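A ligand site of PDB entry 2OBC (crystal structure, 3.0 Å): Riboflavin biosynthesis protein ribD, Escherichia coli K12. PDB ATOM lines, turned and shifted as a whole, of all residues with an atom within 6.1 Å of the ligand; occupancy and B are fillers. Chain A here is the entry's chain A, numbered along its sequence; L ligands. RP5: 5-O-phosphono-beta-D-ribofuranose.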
ATOM      1  N   LYS A 179     -23.905   2.022 -19.857  1.00  0.00           N
ATOM      2  CA  LYS A 179     -24.474   0.673 -19.861  1.00  0.00           C
ATOM      3  C   LYS A 179     -23.541  -0.299 -19.180  1.00  0.00           C
ATOM      4  O   LYS A 179     -22.332  -0.182 -19.313  1.00  0.00           O
ATOM      5  CB  LYS A 179     -24.866   0.203 -21.257  1.00  0.00           C
ATOM      6  CG  LYS A 179     -23.877  -0.740 -21.949  1.00  0.00           C
ATOM      7  CD  LYS A 179     -24.244  -2.202 -21.752  1.00  0.00           C
ATOM      8  CE  LYS A 179     -22.975  -3.077 -21.733  1.00  0.00           C
ATOM      9  NZ  LYS A 179     -22.476  -3.479 -23.097  1.00  0.00           N
ATOM     10  N   MET A 190     -20.874  -9.279 -19.996  1.00  0.00           N
ATOM     11  CA  MET A 190     -21.242  -8.694 -21.286  1.00  0.00           C
ATOM     12  C   MET A 190     -20.061  -7.927 -21.877  1.00  0.00           C
ATOM     13  O   MET A 190     -19.098  -8.529 -22.346  1.00  0.00           O
ATOM     14  CB  MET A 190     -22.457  -7.761 -21.154  1.00  0.00           C
ATOM     15  CG  MET A 190     -23.263  -7.597 -22.442  1.00  0.00           C
ATOM     16  SD  MET A 190     -24.603  -6.150 -22.462  1.00  0.00           S
ATOM     17  CE  MET A 190     -25.883  -6.963 -23.703  1.00  0.00           C
ATOM     18  N   GLU A 194     -16.323  -9.386 -28.286  1.00  0.00           N
ATOM     19  CA  GLU A 194     -17.453  -9.502 -27.368  1.00  0.00           C
ATOM     20  C   GLU A 194     -18.809  -9.241 -28.061  1.00  0.00           C
ATOM     21  O   GLU A 194     -19.495  -8.251 -27.782  1.00  0.00           O
ATOM     22  CB  GLU A 194     -17.250  -8.583 -26.151  1.00  0.00           C
ATOM     23  CG  GLU A 194     -16.149  -9.022 -25.187  1.00  0.00           C
ATOM     24  CD  GLU A 194     -16.508 -10.276 -24.389  1.00  0.00           C
ATOM     25  OE1 GLU A 194     -15.631 -11.155 -24.258  1.00  0.00           O
ATOM     26  OE2 GLU A 194     -17.654 -10.375 -23.893  1.00  0.00           O
ATOM     27  N   SER A 195     -19.167 -10.140 -28.973  1.00  0.00           N
ATOM     28  CA  SER A 195     -20.527 -10.189 -29.543  1.00  0.00           C
ATOM     29  C   SER A 195     -21.080 -11.616 -29.425  1.00  0.00           C
ATOM     30  O   SER A 195     -22.275 -11.853 -29.683  1.00  0.00           O
ATOM     31  CB  SER A 195     -20.544  -9.689 -30.996  1.00  0.00           C
ATOM     32  OG  SER A 195     -20.559  -8.271 -31.029  1.00  0.00           O
ATOM     33  N   TRP A 197     -21.497 -12.518 -26.734  1.00  0.00           N
ATOM     34  CA  TRP A 197     -21.880 -12.131 -25.369  1.00  0.00           C
ATOM     35  C   TRP A 197     -22.579 -13.240 -24.561  1.00  0.00           C
ATOM     36  O   TRP A 197     -23.496 -13.914 -25.042  1.00  0.00           O
ATOM     37  CB  TRP A 197     -22.740 -10.848 -25.379  1.00  0.00           C
ATOM     38  CG  TRP A 197     -21.963  -9.536 -25.314  1.00  0.00           C
ATOM     39  CD1 TRP A 197     -20.699  -9.347 -24.815  1.00  0.00           C
ATOM     40  CD2 TRP A 197     -22.432  -8.236 -25.724  1.00  0.00           C
ATOM     41  NE1 TRP A 197     -20.344  -8.017 -24.907  1.00  0.00           N
ATOM     42  CE2 TRP A 197     -21.381  -7.314 -25.458  1.00  0.00           C
ATOM     43  CE3 TRP A 197     -23.620  -7.760 -26.299  1.00  0.00           C
ATOM     44  CZ2 TRP A 197     -21.492  -5.941 -25.756  1.00  0.00           C
ATOM     45  CZ3 TRP A 197     -23.730  -6.392 -26.583  1.00  0.00           C
ATOM     46  CH2 TRP A 197     -22.671  -5.505 -26.316  1.00  0.00           C
ATOM     47  N   VAL A 207     -29.429  -3.409 -27.168  1.00  0.00           N
ATOM     48  CA  VAL A 207     -28.292  -2.490 -27.181  1.00  0.00           C
ATOM     49  C   VAL A 207     -28.101  -1.790 -28.534  1.00  0.00           C
ATOM     50  O   VAL A 207     -27.820  -0.586 -28.590  1.00  0.00           O
ATOM     51  CB  VAL A 207     -26.990  -3.219 -26.841  1.00  0.00           C
ATOM     52  CG1 VAL A 207     -25.825  -2.239 -26.758  1.00  0.00           C
ATOM     53  CG2 VAL A 207     -27.137  -3.956 -25.542  1.00  0.00           C
ATOM     54  N   GLN A 208     -28.242  -2.558 -29.611  1.00  0.00           N
ATOM     55  CA  GLN A 208     -28.155  -2.020 -30.961  1.00  0.00           C
ATOM     56  C   GLN A 208     -29.177  -0.907 -31.155  1.00  0.00           C
ATOM     57  O   GLN A 208     -28.867   0.115 -31.746  1.00  0.00           O
ATOM     58  CB  GLN A 208     -28.376  -3.122 -31.995  1.00  0.00           C
ATOM     59  CG  GLN A 208     -27.128  -3.907 -32.356  1.00  0.00           C
ATOM     60  CD  GLN A 208     -26.174  -3.108 -33.226  1.00  0.00           C
ATOM     61  OE1 GLN A 208     -26.559  -2.595 -34.278  1.00  0.00           O
ATOM     62  NE2 GLN A 208     -24.917  -3.012 -32.805  1.00  0.00           N
ATOM     63  N   ARG A 211     -27.959   2.155 -29.149  1.00  0.00           N
ATOM     64  CA  ARG A 211     -26.858   2.799 -29.883  1.00  0.00           C
ATOM     65  C   ARG A 211     -27.411   3.633 -31.025  1.00  0.00           C
ATOM     66  O   ARG A 211     -27.072   4.805 -31.188  1.00  0.00           O
ATOM     67  CB  ARG A 211     -25.925   1.767 -30.497  1.00  0.00           C
ATOM     68  CG  ARG A 211     -25.007   1.035 -29.556  1.00  0.00           C
ATOM     69  CD  ARG A 211     -24.267  -0.056 -30.327  1.00  0.00           C
ATOM     70  NE  ARG A 211     -23.185  -0.635 -29.539  1.00  0.00           N
ATOM     71  CZ  ARG A 211     -22.257  -1.443 -30.028  1.00  0.00           C
ATOM     72  NH1 ARG A 211     -22.246  -1.795 -31.307  1.00  0.00           N
ATOM     73  NH2 ARG A 211     -21.305  -1.904 -29.226  1.00  0.00           N
ATOM     74  N   THR A 219     -15.988   5.053 -25.539  1.00  0.00           N
ATOM     75  CA  THR A 219     -15.308   3.883 -25.016  1.00  0.00           C
ATOM     76  C   THR A 219     -13.877   4.239 -24.636  1.00  0.00           C
ATOM     77  O   THR A 219     -13.441   5.381 -24.832  1.00  0.00           O
ATOM     78  CB  THR A 219     -15.281   2.724 -26.028  1.00  0.00           C
ATOM     79  OG1 THR A 219     -14.694   1.566 -25.419  1.00  0.00           O
ATOM     80  CG2 THR A 219     -14.451   3.104 -27.243  1.00  0.00           C
ATOM     81  N   THR A 223     -10.780  -1.253 -23.797  1.00  0.00           N
ATOM     82  CA  THR A 223     -11.861  -1.991 -24.431  1.00  0.00           C
ATOM     83  C   THR A 223     -11.502  -2.209 -25.892  1.00  0.00           C
ATOM     84  O   THR A 223     -11.619  -3.328 -26.404  1.00  0.00           O
ATOM     85  CB  THR A 223     -13.165  -1.202 -24.312  1.00  0.00           C
ATOM     86  OG1 THR A 223     -13.487  -1.031 -22.924  1.00  0.00           O
ATOM     87  CG2 THR A 223     -14.312  -1.896 -25.047  1.00  0.00           C
ATOM     88  N   VAL A 224     -11.023  -1.162 -26.547  1.00  0.00           N
ATOM     89  CA  VAL A 224     -10.658  -1.254 -27.948  1.00  0.00           C
ATOM     90  C   VAL A 224      -9.507  -2.247 -28.120  1.00  0.00           C
ATOM     91  O   VAL A 224      -9.521  -3.061 -29.043  1.00  0.00           O
ATOM     92  CB  VAL A 224     -10.337   0.118 -28.557  1.00  0.00           C
ATOM     93  CG1 VAL A 224      -9.986  -0.013 -30.017  1.00  0.00           C
ATOM     94  CG2 VAL A 224     -11.522   1.050 -28.397  1.00  0.00           C
ATOM     95  N   ASP A 227     -10.851  -6.031 -27.032  1.00  0.00           N
ATOM     96  CA  ASP A 227     -11.916  -6.581 -27.864  1.00  0.00           C
ATOM     97  C   ASP A 227     -11.766  -6.304 -29.365  1.00  0.00           C
ATOM     98  O   ASP A 227     -12.174  -7.118 -30.191  1.00  0.00           O
ATOM     99  CB  ASP A 227     -13.294  -6.114 -27.366  1.00  0.00           C
ATOM    100  CG  ASP A 227     -13.571  -6.530 -25.928  1.00  0.00           C
ATOM    101  OD1 ASP A 227     -14.296  -5.793 -25.209  1.00  0.00           O
ATOM    102  OD2 ASP A 227     -13.050  -7.586 -25.495  1.00  0.00           O
ATOM    103  N   ASP A 228     -11.155  -5.175 -29.714  1.00  0.00           N
ATOM    104  CA  ASP A 228     -11.138  -4.690 -31.101  1.00  0.00           C
ATOM    105  C   ASP A 228     -12.550  -4.599 -31.684  1.00  0.00           C
ATOM    106  O   ASP A 228     -12.814  -5.148 -32.749  1.00  0.00           O
ATOM    107  CB  ASP A 228     -10.211  -5.547 -31.983  1.00  0.00           C
ATOM    108  CG  ASP A 228      -9.837  -4.854 -33.299  1.00  0.00           C
ATOM    109  OD1 ASP A 228     -10.013  -3.609 -33.412  1.00  0.00           O
ATOM    110  OD2 ASP A 228      -9.370  -5.555 -34.233  1.00  0.00           O
ATOM    111  N   PRO A 229     -13.456  -3.897 -30.995  1.00  0.00           N
ATOM    112  CA  PRO A 229     -14.837  -3.750 -31.432  1.00  0.00           C
ATOM    113  C   PRO A 229     -14.957  -2.821 -32.634  1.00  0.00           C
ATOM    114  O   PRO A 229     -13.983  -2.143 -32.984  1.00  0.00           O
ATOM    115  CB  PRO A 229     -15.518  -3.085 -30.238  1.00  0.00           C
ATOM    116  CG  PRO A 229     -14.427  -2.288 -29.599  1.00  0.00           C
ATOM    117  CD  PRO A 229     -13.203  -3.157 -29.740  1.00  0.00           C
ATOM    118  N   ALA A 230     -16.143  -2.774 -33.235  1.00  0.00           N
ATOM    119  CA  ALA A 230     -16.417  -1.871 -34.344  1.00  0.00           C
ATOM    120  C   ALA A 230     -17.267  -0.683 -33.884  1.00  0.00           C
ATOM    121  O   ALA A 230     -17.340   0.348 -34.571  1.00  0.00           O
ATOM    122  CB  ALA A 230     -17.096  -2.608 -35.475  1.00  0.00           C
ATOM    123  N   LEU A 231     -17.894  -0.832 -32.715  1.00  0.00           N
ATOM    124  CA  LEU A 231     -18.759   0.198 -32.129  1.00  0.00           C
ATOM    125  C   LEU A 231     -19.763   0.858 -33.089  1.00  0.00           C
ATOM    126  O   LEU A 231     -20.049   2.048 -32.958  1.00  0.00           O
ATOM    127  CB  LEU A 231     -17.913   1.231 -31.394  1.00  0.00           C
ATOM    128  CG  LEU A 231     -17.280   0.684 -30.117  1.00  0.00           C
ATOM    129  CD1 LEU A 231     -16.767   1.829 -29.279  1.00  0.00           C
ATOM    130  CD2 LEU A 231     -18.279  -0.155 -29.333  1.00  0.00           C
ATOM    131  N   THR A 232     -20.283   0.083 -34.028  1.00  0.00           N
ATOM    132  CA  THR A 232     -21.292   0.564 -34.984  1.00  0.00           C
ATOM    133  C   THR A 232     -22.644  -0.072 -34.740  1.00  0.00           C
ATOM    134  O   THR A 232     -22.795  -1.027 -33.979  1.00  0.00           O
ATOM    135  CB  THR A 232     -20.900   0.262 -36.440  1.00  0.00           C
ATOM    136  OG1 THR A 232     -20.546  -1.108 -36.589  1.00  0.00           O
ATOM    137  CG2 THR A 232     -19.734   1.108 -36.865  1.00  0.00           C
ATOM    138  N   VAL A 233     -23.650   0.481 -35.415  1.00  0.00           N
ATOM    139  CA  VAL A 233     -24.996  -0.073 -35.481  1.00  0.00           C
ATOM    140  C   VAL A 233     -25.097  -0.893 -36.776  1.00  0.00           C
ATOM    141  O   VAL A 233     -24.761  -0.381 -37.853  1.00  0.00           O
ATOM    142  CB  VAL A 233     -26.044   1.042 -35.537  1.00  0.00           C
ATOM    143  CG1 VAL A 233     -27.437   0.484 -35.616  1.00  0.00           C
ATOM    144  CG2 VAL A 233     -25.893   1.954 -34.340  1.00  0.00           C
ATOM    145  N   ARG A 234     -25.523  -2.142 -36.657  1.00  0.00           N
ATOM    146  CA  ARG A 234     -25.749  -2.989 -37.832  1.00  0.00           C
ATOM    147  C   ARG A 234     -27.225  -2.997 -38.107  1.00  0.00           C
ATOM    148  O   ARG A 234     -27.997  -3.556 -37.345  1.00  0.00           O
ATOM    149  CB  ARG A 234     -25.236  -4.415 -37.614  1.00  0.00           C
ATOM    150  CG  ARG A 234     -23.801  -4.664 -38.113  1.00  0.00           C
ATOM    151  CD  ARG A 234     -22.742  -4.067 -37.181  1.00  0.00           C
ATOM    152  NE  ARG A 234     -22.922  -4.564 -35.817  1.00  0.00           N
ATOM    153  CZ  ARG A 234     -22.190  -4.205 -34.765  1.00  0.00           C
ATOM    154  NH1 ARG A 234     -21.196  -3.341 -34.885  1.00  0.00           N
ATOM    155  NH2 ARG A 234     -22.467  -4.730 -33.577  1.00  0.00           N
ATOM    156  N   GLU A 237     -29.662  -5.729 -37.455  1.00  0.00           N
ATOM    157  CA  GLU A 237     -29.996  -6.127 -36.104  1.00  0.00           C
ATOM    158  C   GLU A 237     -31.137  -5.307 -35.498  1.00  0.00           C
ATOM    159  O   GLU A 237     -31.337  -5.314 -34.288  1.00  0.00           O
ATOM    160  CB  GLU A 237     -28.759  -6.097 -35.208  1.00  0.00           C
ATOM    161  CG  GLU A 237     -27.873  -7.341 -35.307  1.00  0.00           C
ATOM    162  CD  GLU A 237     -26.912  -7.478 -34.111  1.00  0.00           C
ATOM    163  OE1 GLU A 237     -26.084  -6.552 -33.887  1.00  0.00           O
ATOM    164  OE2 GLU A 237     -26.983  -8.511 -33.399  1.00  0.00           O
ATOM    165  N   ARG A 270     -10.062  -2.169 -35.866  1.00  0.00           N
ATOM    166  CA  ARG A 270     -11.301  -2.208 -36.615  1.00  0.00           C
ATOM    167  C   ARG A 270     -12.083  -0.940 -36.410  1.00  0.00           C
ATOM    168  O   ARG A 270     -12.797  -0.485 -37.300  1.00  0.00           O
ATOM    169  CB  ARG A 270     -12.143  -3.432 -36.214  1.00  0.00           C
ATOM    170  CG  ARG A 270     -11.508  -4.776 -36.571  1.00  0.00           C
ATOM    171  CD  ARG A 270     -12.224  -5.961 -35.902  1.00  0.00           C
ATOM    172  NE  ARG A 270     -13.499  -6.294 -36.557  1.00  0.00           N
ATOM    173  CZ  ARG A 270     -14.695  -5.835 -36.181  1.00  0.00           C
ATOM    174  NH1 ARG A 270     -14.813  -5.008 -35.153  1.00  0.00           N
ATOM    175  NH2 ARG A 270     -15.784  -6.205 -36.849  1.00  0.00           N
ATOM    176  N   TRP A 324     -23.546   7.189 -25.488  1.00  0.00           N
ATOM    177  CA  TRP A 324     -23.836   5.868 -25.006  1.00  0.00           C
ATOM    178  C   TRP A 324     -22.472   5.244 -24.738  1.00  0.00           C
ATOM    179  O   TRP A 324     -21.698   5.052 -25.679  1.00  0.00           O
ATOM    180  CB  TRP A 324     -24.623   5.067 -26.061  1.00  0.00           C
ATOM    181  CG  TRP A 324     -24.685   3.579 -25.807  1.00  0.00           C
ATOM    182  CD1 TRP A 324     -23.765   2.649 -26.210  1.00  0.00           C
ATOM    183  CD2 TRP A 324     -25.704   2.853 -25.109  1.00  0.00           C
ATOM    184  NE1 TRP A 324     -24.142   1.405 -25.791  1.00  0.00           N
ATOM    185  CE2 TRP A 324     -25.323   1.496 -25.112  1.00  0.00           C
ATOM    186  CE3 TRP A 324     -26.891   3.223 -24.472  1.00  0.00           C
ATOM    187  CZ2 TRP A 324     -26.103   0.505 -24.512  1.00  0.00           C
ATOM    188  CZ3 TRP A 324     -27.658   2.235 -23.856  1.00  0.00           C
ATOM    189  CH2 TRP A 324     -27.268   0.896 -23.884  1.00  0.00           C
ATOM    190  N   GLU A 326     -19.937   2.344 -23.899  1.00  0.00           N
ATOM    191  CA  GLU A 326     -19.596   0.917 -23.841  1.00  0.00           C
ATOM    192  C   GLU A 326     -18.167   0.825 -23.350  1.00  0.00           C
ATOM    193  O   GLU A 326     -17.243   0.604 -24.132  1.00  0.00           O
ATOM    194  CB  GLU A 326     -19.645   0.256 -25.226  1.00  0.00           C
ATOM    195  CG  GLU A 326     -20.918   0.460 -26.013  1.00  0.00           C
ATOM    196  CD  GLU A 326     -21.843  -0.741 -25.982  1.00  0.00           C
ATOM    197  OE1 GLU A 326     -22.577  -0.938 -26.976  1.00  0.00           O
ATOM    198  OE2 GLU A 326     -21.823  -1.479 -24.975  1.00  0.00           O
ATOM    199  N   ALA A 327     -17.979   0.989 -22.048  1.00  0.00           N
ATOM    200  CA  ALA A 327     -16.635   0.868 -21.455  1.00  0.00           C
ATOM    201  C   ALA A 327     -16.513  -0.351 -20.546  1.00  0.00           C
ATOM    202  O   ALA A 327     -17.519  -1.010 -20.239  1.00  0.00           O
ATOM    203  CB  ALA A 327     -16.287   2.128 -20.691  1.00  0.00           C
HETATM  204  C1  RP5 L   1     -17.125  -4.466 -26.123  1.00  0.00           C
HETATM  205  O4  RP5 L   1     -17.843  -5.321 -27.015  1.00  0.00           O
HETATM  206  C2  RP5 L   1     -17.866  -3.136 -26.057  1.00  0.00           C
HETATM  207  O2  RP5 L   1     -18.554  -3.007 -24.807  1.00  0.00           O
HETATM  208  C3  RP5 L   1     -18.826  -3.162 -27.244  1.00  0.00           C
HETATM  209  O3  RP5 L   1     -20.150  -2.812 -26.845  1.00  0.00           O
HETATM  210  C4  RP5 L   1     -18.802  -4.583 -27.793  1.00  0.00           C
HETATM  211  C5  RP5 L   1     -18.472  -4.678 -29.282  1.00  0.00           C
HETATM  212  O5  RP5 L   1     -19.355  -3.869 -30.085  1.00  0.00           O
HETATM  213  P'  RP5 L   1     -19.502  -4.054 -31.677  1.00  0.00           P
HETATM  214  O1X RP5 L   1     -20.624  -5.048 -31.805  1.00  0.00           O
HETATM  215  O2X RP5 L   1     -19.904  -2.679 -32.170  1.00  0.00           O
HETATM  216  O3X RP5 L   1     -18.169  -4.553 -32.182  1.00  0.00           O
HETATM  217  O1  RP5 L   1     -15.838  -4.215 -26.688  1.00  0.00           O
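An oxygen (O4) of the ligand sits close to the backbone carbonyl oxygen of Glu 194. Trp 197 touches the ligand (CZ2 to O3, 3.6 Å). CG2 of Thr 223 touches O1 of the ligand, at 3.2 Å. Pro 229 touches the ligand. Hydrophobic or aromatic side chains within 4 Å of the ligand: Trp 197, Pro 229, Ala 230 and Leu 231. The nearest printed residue that does not touch the ligand is Lys 179 (4.3 Å).
The side-chain amide oxygen (OE1) of Gln 208 sits at hydrogen-bond distance from the backbone NH (N) of Arg 234, 2.6 Å away. NH1 of Arg 211 sits at hydrogen-bond distance from O of Thr 232 (2.8 Å). NH1 of Arg 211 lies close to NE2 of Gln 208 (3.3 Å). OE2 of Glu 326 lies within salt-bridge range of NZ of Lys 179 (2.8 Å). The side-chain carboxylate of Glu 326 sits at hydrogen-bond distance from the indole nitrogen of Trp 324, at 3.1 Å. O of Thr 232 lies within hydrogen-bond range of NE2 of Gln 208, at 3.1 Å. O of Glu 194 lies within hydrogen-bond range of NE1 of Trp 197, 3.0 Å away. The indole nitrogen of Trp 197 sits at hydrogen-bond distance from the backbone carbonyl oxygen of Met 190, 2.9 Å away.
NH2 of Arg 234 lies within salt-bridge range of O1X of the ligand (2.6 Å). An oxygen (O2X) of the ligand is in salt-bridge range of the guanidinium group of Arg 211 (2.6 Å). An oxygen (O1) of the ligand is in hydrogen-bond range of the side-chain carboxylate (OD1) of Asp 227 (2.7 Å). The backbone NH (N) of Leu 231 lies within hydrogen-bond range of an oxygen (O2X) of the ligand, at 2.8 Å. The side-chain carboxylate (OE2) of Glu 326 sits close to an oxygen (O3) of the ligand, at 2.8 Å. The backbone NH (N) of Ala 230 sits at hydrogen-bond distance from an oxygen (O3X) of the ligand, 2.9 Å away. An oxygen (O1X) of the ligand sits at hydrogen-bond distance from the side-chain hydroxyl of Ser 195, 3.3 Å away. An oxygen (O2X) of the ligand is in hydrogen-bond range of the backbone NH (N) of Thr 232 (3.4 Å).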
